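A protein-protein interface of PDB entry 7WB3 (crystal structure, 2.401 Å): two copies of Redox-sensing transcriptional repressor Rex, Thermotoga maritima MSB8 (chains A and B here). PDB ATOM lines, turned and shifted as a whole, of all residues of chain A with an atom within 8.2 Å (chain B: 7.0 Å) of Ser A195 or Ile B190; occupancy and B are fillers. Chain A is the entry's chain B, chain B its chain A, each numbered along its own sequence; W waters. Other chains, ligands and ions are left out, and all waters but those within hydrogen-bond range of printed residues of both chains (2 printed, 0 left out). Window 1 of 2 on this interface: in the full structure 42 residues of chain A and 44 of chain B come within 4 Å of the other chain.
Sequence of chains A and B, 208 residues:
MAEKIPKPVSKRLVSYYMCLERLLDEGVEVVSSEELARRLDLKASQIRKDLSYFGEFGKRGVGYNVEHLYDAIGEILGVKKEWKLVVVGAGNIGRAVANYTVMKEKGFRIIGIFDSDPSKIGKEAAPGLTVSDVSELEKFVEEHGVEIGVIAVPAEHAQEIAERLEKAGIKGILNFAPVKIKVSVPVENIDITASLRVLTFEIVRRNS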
ATOM      1  N   LYS A  11      12.093 -29.392   9.022  1.00  0.00           N
ATOM      2  CA  LYS A  11      13.016 -29.629  10.126  1.00  0.00           C
ATOM      3  C   LYS A  11      12.274 -29.655  11.457  1.00  0.00           C
ATOM      4  O   LYS A  11      12.483 -30.551  12.282  1.00  0.00           O
ATOM      5  CB  LYS A  11      14.108 -28.558  10.133  1.00  0.00           C
ATOM      6  CG  LYS A  11      15.403 -28.984  10.802  1.00  0.00           C
ATOM      7  CD  LYS A  11      16.470 -27.910  10.655  1.00  0.00           C
ATOM      8  CE  LYS A  11      17.726 -28.260  11.437  1.00  0.00           C
ATOM      9  NZ  LYS A  11      18.365 -29.505  10.931  1.00  0.00           N
ATOM     10  N   PHE A 176      27.723 -36.769   3.084  1.00  0.00           N
ATOM     11  CA  PHE A 176      28.654 -36.345   4.122  1.00  0.00           C
ATOM     12  C   PHE A 176      29.872 -35.610   3.578  1.00  0.00           C
ATOM     13  O   PHE A 176      30.577 -34.957   4.356  1.00  0.00           O
ATOM     14  CB  PHE A 176      29.129 -37.556   4.937  1.00  0.00           C
ATOM     15  CG  PHE A 176      28.139 -38.024   5.965  1.00  0.00           C
ATOM     16  CD1 PHE A 176      27.180 -38.968   5.644  1.00  0.00           C
ATOM     17  CD2 PHE A 176      28.172 -37.525   7.257  1.00  0.00           C
ATOM     18  CE1 PHE A 176      26.269 -39.402   6.589  1.00  0.00           C
ATOM     19  CE2 PHE A 176      27.265 -37.954   8.206  1.00  0.00           C
ATOM     20  CZ  PHE A 176      26.312 -38.895   7.870  1.00  0.00           C
ATOM     21  N   ASN A 189      22.607 -32.699   3.119  1.00  0.00           N
ATOM     22  CA  ASN A 189      24.041 -32.670   3.361  1.00  0.00           C
ATOM     23  C   ASN A 189      24.319 -32.546   4.852  1.00  0.00           C
ATOM     24  O   ASN A 189      23.614 -31.831   5.571  1.00  0.00           O
ATOM     25  CB  ASN A 189      24.707 -31.510   2.614  1.00  0.00           C
ATOM     26  CG  ASN A 189      24.486 -31.577   1.115  1.00  0.00           C
ATOM     27  OD1 ASN A 189      25.176 -32.310   0.407  1.00  0.00           O
ATOM     28  ND2 ASN A 189      23.524 -30.805   0.625  1.00  0.00           N
ATOM     29  N   ILE A 190      25.346 -33.257   5.308  1.00  0.00           N
ATOM     30  CA  ILE A 190      25.874 -33.128   6.659  1.00  0.00           C
ATOM     31  C   ILE A 190      27.355 -32.807   6.521  1.00  0.00           C
ATOM     32  O   ILE A 190      28.159 -33.685   6.184  1.00  0.00           O
ATOM     33  CB  ILE A 190      25.658 -34.399   7.492  1.00  0.00           C
ATOM     34  CG1 ILE A 190      24.168 -34.606   7.771  1.00  0.00           C
ATOM     35  CG2 ILE A 190      26.448 -34.324   8.791  1.00  0.00           C
ATOM     36  CD1 ILE A 190      23.871 -35.820   8.622  1.00  0.00           C
ATOM     37  N   ASP A 191      27.716 -31.551   6.769  1.00  0.00           N
ATOM     38  CA  ASP A 191      29.085 -31.072   6.600  1.00  0.00           C
ATOM     39  C   ASP A 191      29.653 -30.781   7.985  1.00  0.00           C
ATOM     40  O   ASP A 191      29.434 -29.701   8.543  1.00  0.00           O
ATOM     41  CB  ASP A 191      29.118 -29.839   5.702  1.00  0.00           C
ATOM     42  CG  ASP A 191      30.517 -29.500   5.223  1.00  0.00           C
ATOM     43  OD1 ASP A 191      31.490 -29.806   5.946  1.00  0.00           O
ATOM     44  OD2 ASP A 191      30.644 -28.924   4.122  1.00  0.00           O
ATOM     45  N   ILE A 192      30.395 -31.748   8.530  1.00  0.00           N
ATOM     46  CA  ILE A 192      30.885 -31.635   9.902  1.00  0.00           C
ATOM     47  C   ILE A 192      31.827 -30.445  10.038  1.00  0.00           C
ATOM     48  O   ILE A 192      31.721 -29.651  10.981  1.00  0.00           O
ATOM     49  CB  ILE A 192      31.565 -32.946  10.337  1.00  0.00           C
ATOM     50  CG1 ILE A 192      30.527 -34.063  10.475  1.00  0.00           C
ATOM     51  CG2 ILE A 192      32.324 -32.744  11.641  1.00  0.00           C
ATOM     52  CD1 ILE A 192      31.125 -35.429  10.747  1.00  0.00           C
ATOM     53  N   THR A 193      32.770 -30.308   9.104  1.00  0.00           N
ATOM     54  CA  THR A 193      33.728 -29.210   9.183  1.00  0.00           C
ATOM     55  C   THR A 193      33.033 -27.860   9.064  1.00  0.00           C
ATOM     56  O   THR A 193      33.387 -26.905   9.767  1.00  0.00           O
ATOM     57  CB  THR A 193      34.798 -29.360   8.101  1.00  0.00           C
ATOM     58  OG1 THR A 193      35.581 -30.531   8.365  1.00  0.00           O
ATOM     59  CG2 THR A 193      35.709 -28.140   8.082  1.00  0.00           C
ATOM     60  N   ALA A 194      32.044 -27.756   8.176  1.00  0.00           N
ATOM     61  CA  ALA A 194      31.292 -26.510   8.060  1.00  0.00           C
ATOM     62  C   ALA A 194      30.597 -26.164   9.371  1.00  0.00           C
ATOM     63  O   ALA A 194      30.495 -24.987   9.737  1.00  0.00           O
ATOM     64  CB  ALA A 194      30.280 -26.609   6.919  1.00  0.00           C
ATOM     65  N   SER A 195      30.109 -27.177  10.091  1.00  0.00           N
ATOM     66  CA  SER A 195      29.465 -26.929  11.377  1.00  0.00           C
ATOM     67  C   SER A 195      30.458 -26.366  12.385  1.00  0.00           C
ATOM     68  O   SER A 195      30.161 -25.397  13.093  1.00  0.00           O
ATOM     69  CB  SER A 195      28.831 -28.217  11.904  1.00  0.00           C
ATOM     70  OG  SER A 195      27.740 -28.615  11.093  1.00  0.00           O
ATOM     71  N   LEU A 196      31.647 -26.968  12.470  1.00  0.00           N
ATOM     72  CA  LEU A 196      32.680 -26.440  13.354  1.00  0.00           C
ATOM     73  C   LEU A 196      32.990 -24.985  13.026  1.00  0.00           C
ATOM     74  O   LEU A 196      33.145 -24.154  13.930  1.00  0.00           O
ATOM     75  CB  LEU A 196      33.945 -27.292  13.254  1.00  0.00           C
ATOM     76  CG  LEU A 196      33.903 -28.670  13.919  1.00  0.00           C
ATOM     77  CD1 LEU A 196      35.116 -29.493  13.522  1.00  0.00           C
ATOM     78  CD2 LEU A 196      33.825 -28.531  15.431  1.00  0.00           C
ATOM     79  N   ARG A 197      33.080 -24.656  11.737  1.00  0.00           N
ATOM     80  CA  ARG A 197      33.408 -23.290  11.343  1.00  0.00           C
ATOM     81  C   ARG A 197      32.241 -22.341  11.574  1.00  0.00           C
ATOM     82  O   ARG A 197      32.453 -21.144  11.799  1.00  0.00           O
ATOM     83  CB  ARG A 197      33.855 -23.266   9.882  1.00  0.00           C
ATOM     84  CG  ARG A 197      35.258 -23.819   9.689  1.00  0.00           C
ATOM     85  CD  ARG A 197      35.594 -24.047   8.227  1.00  0.00           C
ATOM     86  NE  ARG A 197      36.987 -24.453   8.062  1.00  0.00           N
ATOM     87  CZ  ARG A 197      37.486 -24.984   6.951  1.00  0.00           C
ATOM     88  NH1 ARG A 197      36.704 -25.184   5.899  1.00  0.00           N
ATOM     89  NH2 ARG A 197      38.767 -25.321   6.896  1.00  0.00           N
ATOM     90  N   VAL A 198      31.006 -22.844  11.519  1.00  0.00           N
ATOM     91  CA  VAL A 198      29.876 -22.045  11.977  1.00  0.00           C
ATOM     92  C   VAL A 198      29.952 -21.841  13.483  1.00  0.00           C
ATOM     93  O   VAL A 198      29.570 -20.782  13.996  1.00  0.00           O
ATOM     94  CB  VAL A 198      28.547 -22.704  11.565  1.00  0.00           C
ATOM     95  CG1 VAL A 198      27.373 -21.944  12.163  1.00  0.00           C
ATOM     96  CG2 VAL A 198      28.433 -22.766  10.051  1.00  0.00           C
ATOM     97  N   LEU A 199      30.452 -22.841  14.212  1.00  0.00           N
ATOM     98  CA  LEU A 199      30.581 -22.722  15.660  1.00  0.00           C
ATOM     99  C   LEU A 199      31.645 -21.697  16.037  1.00  0.00           C
ATOM    100  O   LEU A 199      31.427 -20.858  16.918  1.00  0.00           O
ATOM    101  CB  LEU A 199      30.907 -24.087  16.270  1.00  0.00           C
ATOM    102  CG  LEU A 199      31.063 -24.143  17.790  1.00  0.00           C
ATOM    103  CD1 LEU A 199      29.831 -23.587  18.485  1.00  0.00           C
ATOM    104  CD2 LEU A 199      31.340 -25.571  18.242  1.00  0.00           C
ATOM    105  N   THR A 200      32.810 -21.756  15.388  1.00  0.00           N
ATOM    106  CA  THR A 200      33.855 -20.782  15.682  1.00  0.00           C
ATOM    107  C   THR A 200      33.394 -19.370  15.347  1.00  0.00           C
ATOM    108  O   THR A 200      33.727 -18.414  16.057  1.00  0.00           O
ATOM    109  CB  THR A 200      35.136 -21.123  14.918  1.00  0.00           C
ATOM    110  OG1 THR A 200      34.868 -21.138  13.512  1.00  0.00           O
ATOM    111  CG2 THR A 200      35.663 -22.486  15.344  1.00  0.00           C
ATOM    112  N   PHE A 201      32.619 -19.219  14.270  1.00  0.00           N
ATOM    113  CA  PHE A 201      32.042 -17.919  13.947  1.00  0.00           C
ATOM    114  C   PHE A 201      31.254 -17.367  15.126  1.00  0.00           C
ATOM    115  O   PHE A 201      31.455 -16.221  15.543  1.00  0.00           O
ATOM    116  CB  PHE A 201      31.150 -18.038  12.710  1.00  0.00           C
ATOM    117  CG  PHE A 201      30.323 -16.813  12.438  1.00  0.00           C
ATOM    118  CD1 PHE A 201      30.842 -15.756  11.710  1.00  0.00           C
ATOM    119  CD2 PHE A 201      29.023 -16.722  12.908  1.00  0.00           C
ATOM    120  CE1 PHE A 201      30.082 -14.629  11.458  1.00  0.00           C
ATOM    121  CE2 PHE A 201      28.257 -15.597  12.658  1.00  0.00           C
ATOM    122  CZ  PHE A 201      28.787 -14.550  11.932  1.00  0.00           C
ATOM    123  N   GLU A 202      30.350 -18.176  15.680  1.00  0.00           N
ATOM    124  CA  GLU A 202      29.540 -17.725  16.806  1.00  0.00           C
ATOM    125  C   GLU A 202      30.386 -17.485  18.048  1.00  0.00           C
ATOM    126  O   GLU A 202      30.087 -16.581  18.835  1.00  0.00           O
ATOM    127  CB  GLU A 202      28.442 -18.746  17.099  1.00  0.00           C
ATOM    128  CG  GLU A 202      27.418 -18.893  15.985  1.00  0.00           C
ATOM    129  CD  GLU A 202      26.501 -20.086  16.186  1.00  0.00           C
ATOM    130  OE1 GLU A 202      26.769 -20.899  17.096  1.00  0.00           O
ATOM    131  OE2 GLU A 202      25.511 -20.211  15.435  1.00  0.00           O
ATOM    132  N   LYS B  11      26.488 -19.643   7.453  1.00  0.00           N
ATOM    133  CA  LYS B  11      26.600 -20.887   6.702  1.00  0.00           C
ATOM    134  C   LYS B  11      27.170 -20.638   5.311  1.00  0.00           C
ATOM    135  O   LYS B  11      28.088 -21.338   4.868  1.00  0.00           O
ATOM    136  CB  LYS B  11      25.233 -21.567   6.619  1.00  0.00           C
ATOM    137  CG  LYS B  11      25.292 -23.073   6.426  1.00  0.00           C
ATOM    138  CD  LYS B  11      23.898 -23.683   6.484  1.00  0.00           C
ATOM    139  CE  LYS B  11      23.924 -25.167   6.162  1.00  0.00           C
ATOM    140  NZ  LYS B  11      24.716 -25.937   7.161  1.00  0.00           N
ATOM    141  N   VAL B  14      30.925 -19.838   5.259  1.00  0.00           N
ATOM    142  CA  VAL B  14      31.774 -21.025   5.287  1.00  0.00           C
ATOM    143  C   VAL B  14      31.895 -21.627   3.894  1.00  0.00           C
ATOM    144  O   VAL B  14      32.946 -22.157   3.519  1.00  0.00           O
ATOM    145  CB  VAL B  14      31.228 -22.048   6.302  1.00  0.00           C
ATOM    146  CG1 VAL B  14      32.092 -23.301   6.308  1.00  0.00           C
ATOM    147  CG2 VAL B  14      31.159 -21.433   7.688  1.00  0.00           C
ATOM    148  N   PHE B 108      41.838 -27.562  13.762  1.00  0.00           N
ATOM    149  CA  PHE B 108      41.160 -28.146  14.912  1.00  0.00           C
ATOM    150  C   PHE B 108      41.987 -29.329  15.393  1.00  0.00           C
ATOM    151  O   PHE B 108      42.172 -30.301  14.653  1.00  0.00           O
ATOM    152  CB  PHE B 108      39.740 -28.587  14.548  1.00  0.00           C
ATOM    153  CG  PHE B 108      38.879 -27.475  14.019  1.00  0.00           C
ATOM    154  CD1 PHE B 108      38.146 -26.676  14.877  1.00  0.00           C
ATOM    155  CD2 PHE B 108      38.809 -27.226  12.658  1.00  0.00           C
ATOM    156  CE1 PHE B 108      37.357 -25.652  14.389  1.00  0.00           C
ATOM    157  CE2 PHE B 108      38.023 -26.204  12.165  1.00  0.00           C
ATOM    158  CZ  PHE B 108      37.296 -25.416  13.031  1.00  0.00           C
ATOM    159  N   LEU B 174      29.819 -28.883  19.804  1.00  0.00           N
ATOM    160  CA  LEU B 174      29.276 -29.563  18.636  1.00  0.00           C
ATOM    161  C   LEU B 174      28.540 -30.806  19.122  1.00  0.00           C
ATOM    162  O   LEU B 174      29.161 -31.722  19.671  1.00  0.00           O
ATOM    163  CB  LEU B 174      30.381 -29.938  17.647  1.00  0.00           C
ATOM    164  CG  LEU B 174      29.915 -30.692  16.400  1.00  0.00           C
ATOM    165  CD1 LEU B 174      28.943 -29.845  15.590  1.00  0.00           C
ATOM    166  CD2 LEU B 174      31.099 -31.123  15.548  1.00  0.00           C
ATOM    167  N   ASN B 175      27.225 -30.833  18.922  1.00  0.00           N
ATOM    168  CA  ASN B 175      26.349 -31.823  19.537  1.00  0.00           C
ATOM    169  C   ASN B 175      25.837 -32.796  18.482  1.00  0.00           C
ATOM    170  O   ASN B 175      25.213 -32.381  17.499  1.00  0.00           O
ATOM    171  CB  ASN B 175      25.182 -31.137  20.246  1.00  0.00           C
ATOM    172  CG  ASN B 175      24.189 -32.120  20.822  1.00  0.00           C
ATOM    173  OD1 ASN B 175      24.551 -33.232  21.209  1.00  0.00           O
ATOM    174  ND2 ASN B 175      22.925 -31.718  20.877  1.00  0.00           N
ATOM    175  N   PHE B 176      26.094 -34.087  18.697  1.00  0.00           N
ATOM    176  CA  PHE B 176      25.594 -35.135  17.817  1.00  0.00           C
ATOM    177  C   PHE B 176      24.365 -35.851  18.363  1.00  0.00           C
ATOM    178  O   PHE B 176      23.685 -36.544  17.599  1.00  0.00           O
ATOM    179  CB  PHE B 176      26.686 -36.176  17.547  1.00  0.00           C
ATOM    180  CG  PHE B 176      27.691 -35.759  16.511  1.00  0.00           C
ATOM    181  CD1 PHE B 176      28.836 -35.070  16.869  1.00  0.00           C
ATOM    182  CD2 PHE B 176      27.495 -36.073  15.175  1.00  0.00           C
ATOM    183  CE1 PHE B 176      29.765 -34.694  15.911  1.00  0.00           C
ATOM    184  CE2 PHE B 176      28.416 -35.700  14.216  1.00  0.00           C
ATOM    185  CZ  PHE B 176      29.553 -35.010  14.584  1.00  0.00           C
ATOM    186  N   ALA B 177      24.063 -35.703  19.656  1.00  0.00           N
ATOM    187  CA  ALA B 177      22.980 -36.458  20.276  1.00  0.00           C
ATOM    188  C   ALA B 177      21.625 -35.865  19.892  1.00  0.00           C
ATOM    189  O   ALA B 177      21.461 -34.641  19.880  1.00  0.00           O
ATOM    190  CB  ALA B 177      23.123 -36.462  21.793  1.00  0.00           C
ATOM    191  N   PRO B 178      20.630 -36.708  19.611  1.00  0.00           N
ATOM    192  CA  PRO B 178      19.330 -36.194  19.164  1.00  0.00           C
ATOM    193  C   PRO B 178      18.530 -35.578  20.303  1.00  0.00           C
ATOM    194  O   PRO B 178      17.480 -36.107  20.681  1.00  0.00           O
ATOM    195  CB  PRO B 178      18.643 -37.444  18.597  1.00  0.00           C
ATOM    196  CG  PRO B 178      19.221 -38.569  19.405  1.00  0.00           C
ATOM    197  CD  PRO B 178      20.655 -38.180  19.689  1.00  0.00           C
ATOM    198  N   GLU B 188      26.189 -25.885  17.980  1.00  0.00           N
ATOM    199  CA  GLU B 188      25.816 -26.362  16.656  1.00  0.00           C
ATOM    200  C   GLU B 188      25.467 -27.841  16.751  1.00  0.00           C
ATOM    201  O   GLU B 188      26.230 -28.627  17.324  1.00  0.00           O
ATOM    202  CB  GLU B 188      26.945 -26.140  15.648  1.00  0.00           C
ATOM    203  CG  GLU B 188      26.990 -24.732  15.083  1.00  0.00           C
ATOM    204  CD  GLU B 188      25.698 -24.347  14.386  1.00  0.00           C
ATOM    205  OE1 GLU B 188      25.142 -25.196  13.657  1.00  0.00           O
ATOM    206  OE2 GLU B 188      25.238 -23.200  14.569  1.00  0.00           O
ATOM    207  N   ASN B 189      24.316 -28.214  16.200  1.00  0.00           N
ATOM    208  CA  ASN B 189      23.813 -29.576  16.281  1.00  0.00           C
ATOM    209  C   ASN B 189      23.910 -30.259  14.925  1.00  0.00           C
ATOM    210  O   ASN B 189      23.666 -29.639  13.885  1.00  0.00           O
ATOM    211  CB  ASN B 189      22.359 -29.598  16.765  1.00  0.00           C
ATOM    212  CG  ASN B 189      22.185 -28.944  18.121  1.00  0.00           C
ATOM    213  OD1 ASN B 189      22.444 -29.556  19.158  1.00  0.00           O
ATOM    214  ND2 ASN B 189      21.738 -27.693  18.122  1.00  0.00           N
ATOM    215  N   ILE B 190      24.275 -31.537  14.948  1.00  0.00           N
ATOM    216  CA  ILE B 190      24.246 -32.405  13.778  1.00  0.00           C
ATOM    217  C   ILE B 190      23.400 -33.614  14.149  1.00  0.00           C
ATOM    218  O   ILE B 190      23.846 -34.482  14.911  1.00  0.00           O
ATOM    219  CB  ILE B 190      25.652 -32.827  13.333  1.00  0.00           C
ATOM    220  CG1 ILE B 190      26.424 -31.620  12.794  1.00  0.00           C
ATOM    221  CG2 ILE B 190      25.571 -33.929  12.287  1.00  0.00           C
ATOM    222  CD1 ILE B 190      27.808 -31.954  12.290  1.00  0.00           C
ATOM    223  N   ASP B 191      22.180 -33.672  13.622  1.00  0.00           N
ATOM    224  CA  ASP B 191      21.223 -34.727  13.952  1.00  0.00           C
ATOM    225  C   ASP B 191      21.049 -35.607  12.717  1.00  0.00           C
ATOM    226  O   ASP B 191      20.274 -35.281  11.813  1.00  0.00           O
ATOM    227  CB  ASP B 191      19.896 -34.129  14.415  1.00  0.00           C
ATOM    228  CG  ASP B 191      18.995 -35.152  15.080  1.00  0.00           C
ATOM    229  OD1 ASP B 191      19.087 -36.347  14.731  1.00  0.00           O
ATOM    230  OD2 ASP B 191      18.193 -34.757  15.953  1.00  0.00           O
ATOM    231  N   ILE B 192      21.773 -36.728  12.689  1.00  0.00           N
ATOM    232  CA  ILE B 192      21.787 -37.582  11.503  1.00  0.00           C
ATOM    233  C   ILE B 192      20.396 -38.140  11.225  1.00  0.00           C
ATOM    234  O   ILE B 192      19.916 -38.118  10.085  1.00  0.00           O
ATOM    235  CB  ILE B 192      22.824 -38.708  11.666  1.00  0.00           C
ATOM    236  CG1 ILE B 192      24.243 -38.131  11.641  1.00  0.00           C
ATOM    237  CG2 ILE B 192      22.646 -39.761  10.580  1.00  0.00           C
ATOM    238  CD1 ILE B 192      25.324 -39.143  11.953  1.00  0.00           C
ATOM    239  N   THR B 193      19.727 -38.652  12.260  1.00  0.00           N
ATOM    240  CA  THR B 193      18.401 -39.226  12.056  1.00  0.00           C
ATOM    241  C   THR B 193      17.412 -38.170  11.581  1.00  0.00           C
ATOM    242  O   THR B 193      16.579 -38.438  10.706  1.00  0.00           O
ATOM    243  CB  THR B 193      17.903 -39.885  13.342  1.00  0.00           C
ATOM    244  OG1 THR B 193      18.730 -41.014  13.653  1.00  0.00           O
ATOM    245  CG2 THR B 193      16.461 -40.353  13.174  1.00  0.00           C
ATOM    246  N   ALA B 194      17.485 -36.964  12.144  1.00  0.00           N
ATOM    247  CA  ALA B 194      16.613 -35.888  11.685  1.00  0.00           C
ATOM    248  C   ALA B 194      16.853 -35.578  10.212  1.00  0.00           C
ATOM    249  O   ALA B 194      15.910 -35.271   9.474  1.00  0.00           O
ATOM    250  CB  ALA B 194      16.821 -34.639  12.541  1.00  0.00           C
ATOM    251  N   SER B 195      18.108 -35.659   9.765  1.00  0.00           N
ATOM    252  CA  SER B 195      18.410 -35.410   8.359  1.00  0.00           C
ATOM    253  C   SER B 195      17.759 -36.459   7.466  1.00  0.00           C
ATOM    254  O   SER B 195      17.147 -36.127   6.444  1.00  0.00           O
ATOM    255  CB  SER B 195      19.923 -35.381   8.144  1.00  0.00           C
ATOM    256  OG  SER B 195      20.506 -34.257   8.780  1.00  0.00           O
HETATM  257  O   HOH W   1      25.407 -27.738  12.102  1.00  0.00           O
HETATM  258  O   HOH W   2      21.135 -32.091   7.094  1.00  0.00           O
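The side-chain carboxylate of Glu B188 lies close to the side-chain carboxylate of Glu A202, at 3.1 Å.
The backbone carbonyl oxygen of Leu A196 sits close to the side-chain hydroxyl of Thr A200 (3.5 Å). O of Asn B175 sits at hydrogen-bond distance from N of Ile B190 (2.8 Å). The backbone carbonyl oxygen (O) of Asp A191 is in hydrogen-bond range of the side-chain hydroxyl (OG) of Ser A195, at 3.2 Å. The side-chain carboxylate (OD1) of Asp A191 is in hydrogen-bond range of the backbone NH (N) of Ala A194. OG1 of Thr A200 sits at hydrogen-bond distance from O of Arg A197 (3.0 Å). N of Asn B175 sits at hydrogen-bond distance from O of Glu B188, 2.9 Å away.
Among the printed residues, merely in contact across the chains: Ile A190 with Ile B190 (3.6 Å), Ile A190 with Ile B192 (3.8 Å), Ile A190 with Ser B195 (3.7 Å), Ile A192 with Ile B190 (3.9 Å), Ala A194 with Val B14 (3.7 Å), Ser A195 with Glu B188 (3.8 Å), Ser A195 with Ile B190 (3.5 Å), Leu A196 with Phe B108 (3.8 Å), Leu A196 with Leu B174 (3.8 Å), Arg A197 with Val B14 (3.9 Å), Val A198 with Val B14 (3.8 Å), Val A198 with Glu B188 (3.5 Å), Leu A199 with Leu B174 (3.97 Å) and Thr A200 with Phe B108 (3.7 Å).
Of chain B, only Glu B188 and Ile B190 come within 4 Å of Ser A195. Of chain A, only Ile A190, Ile A192 and Ser A195 come within 4 Å of Ile B190. Printed residues of chain A within 4 Å of Ser B195: Ile A190 (3.7 Å). Printed residues of chain B within 4 Å of Arg A197: Val B14. Of the printed residues of chain B, Ile A192 touches Ile B190. Of the printed residues of chain A, Leu B174 touches Leu A196 (3.8 Å) and Leu A199 (3.97 Å). The nearest printed residue of chain A that does not touch Glu B188 is Leu A199 (4.04 Å).
Printed residues of chain A that touch a printed residue of chain B: Ile A190, Ile A192, Ala A194, Ser A195, Leu A196, Arg A197, Val A198, Leu A199, Thr A200 and Glu A202. Hydrophobic or aromatic side chains of chain A that line the printed part of chain B: Ile A190, Ile A192, Ala A194, Leu A196, Val A198 and Leu A199. Hydrophobic or aromatic side chains of chain B that line the printed part of chain A: Val B14, Phe B108, Leu B174, Ile B190 and Ile B192.
Ile A190 touches its own counterpart, Ile B190. Ile A190 touches Ile B192, and with the chains exchanged Ile A192 touches Ile B190. Ile A190 touches Ser B195, and with the chains exchanged Ser A195 touches Ile B190. Positions printed for both chains: 11, 176, 189, 190, 191, 192, 193, 194 and 195.
Water W1 lies within hydrogen-bond range of the side-chain hydroxyl of Ser A195 (2.7 Å), the side-chain carboxylate of Glu B188 (3.0 Å) and the backbone carbonyl oxygen of Asn B189 (3.1 Å). Water W2 lies within hydrogen-bond range of OG of Ser B195 (2.8 Å) and O of Asn A189 (2.9 Å).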
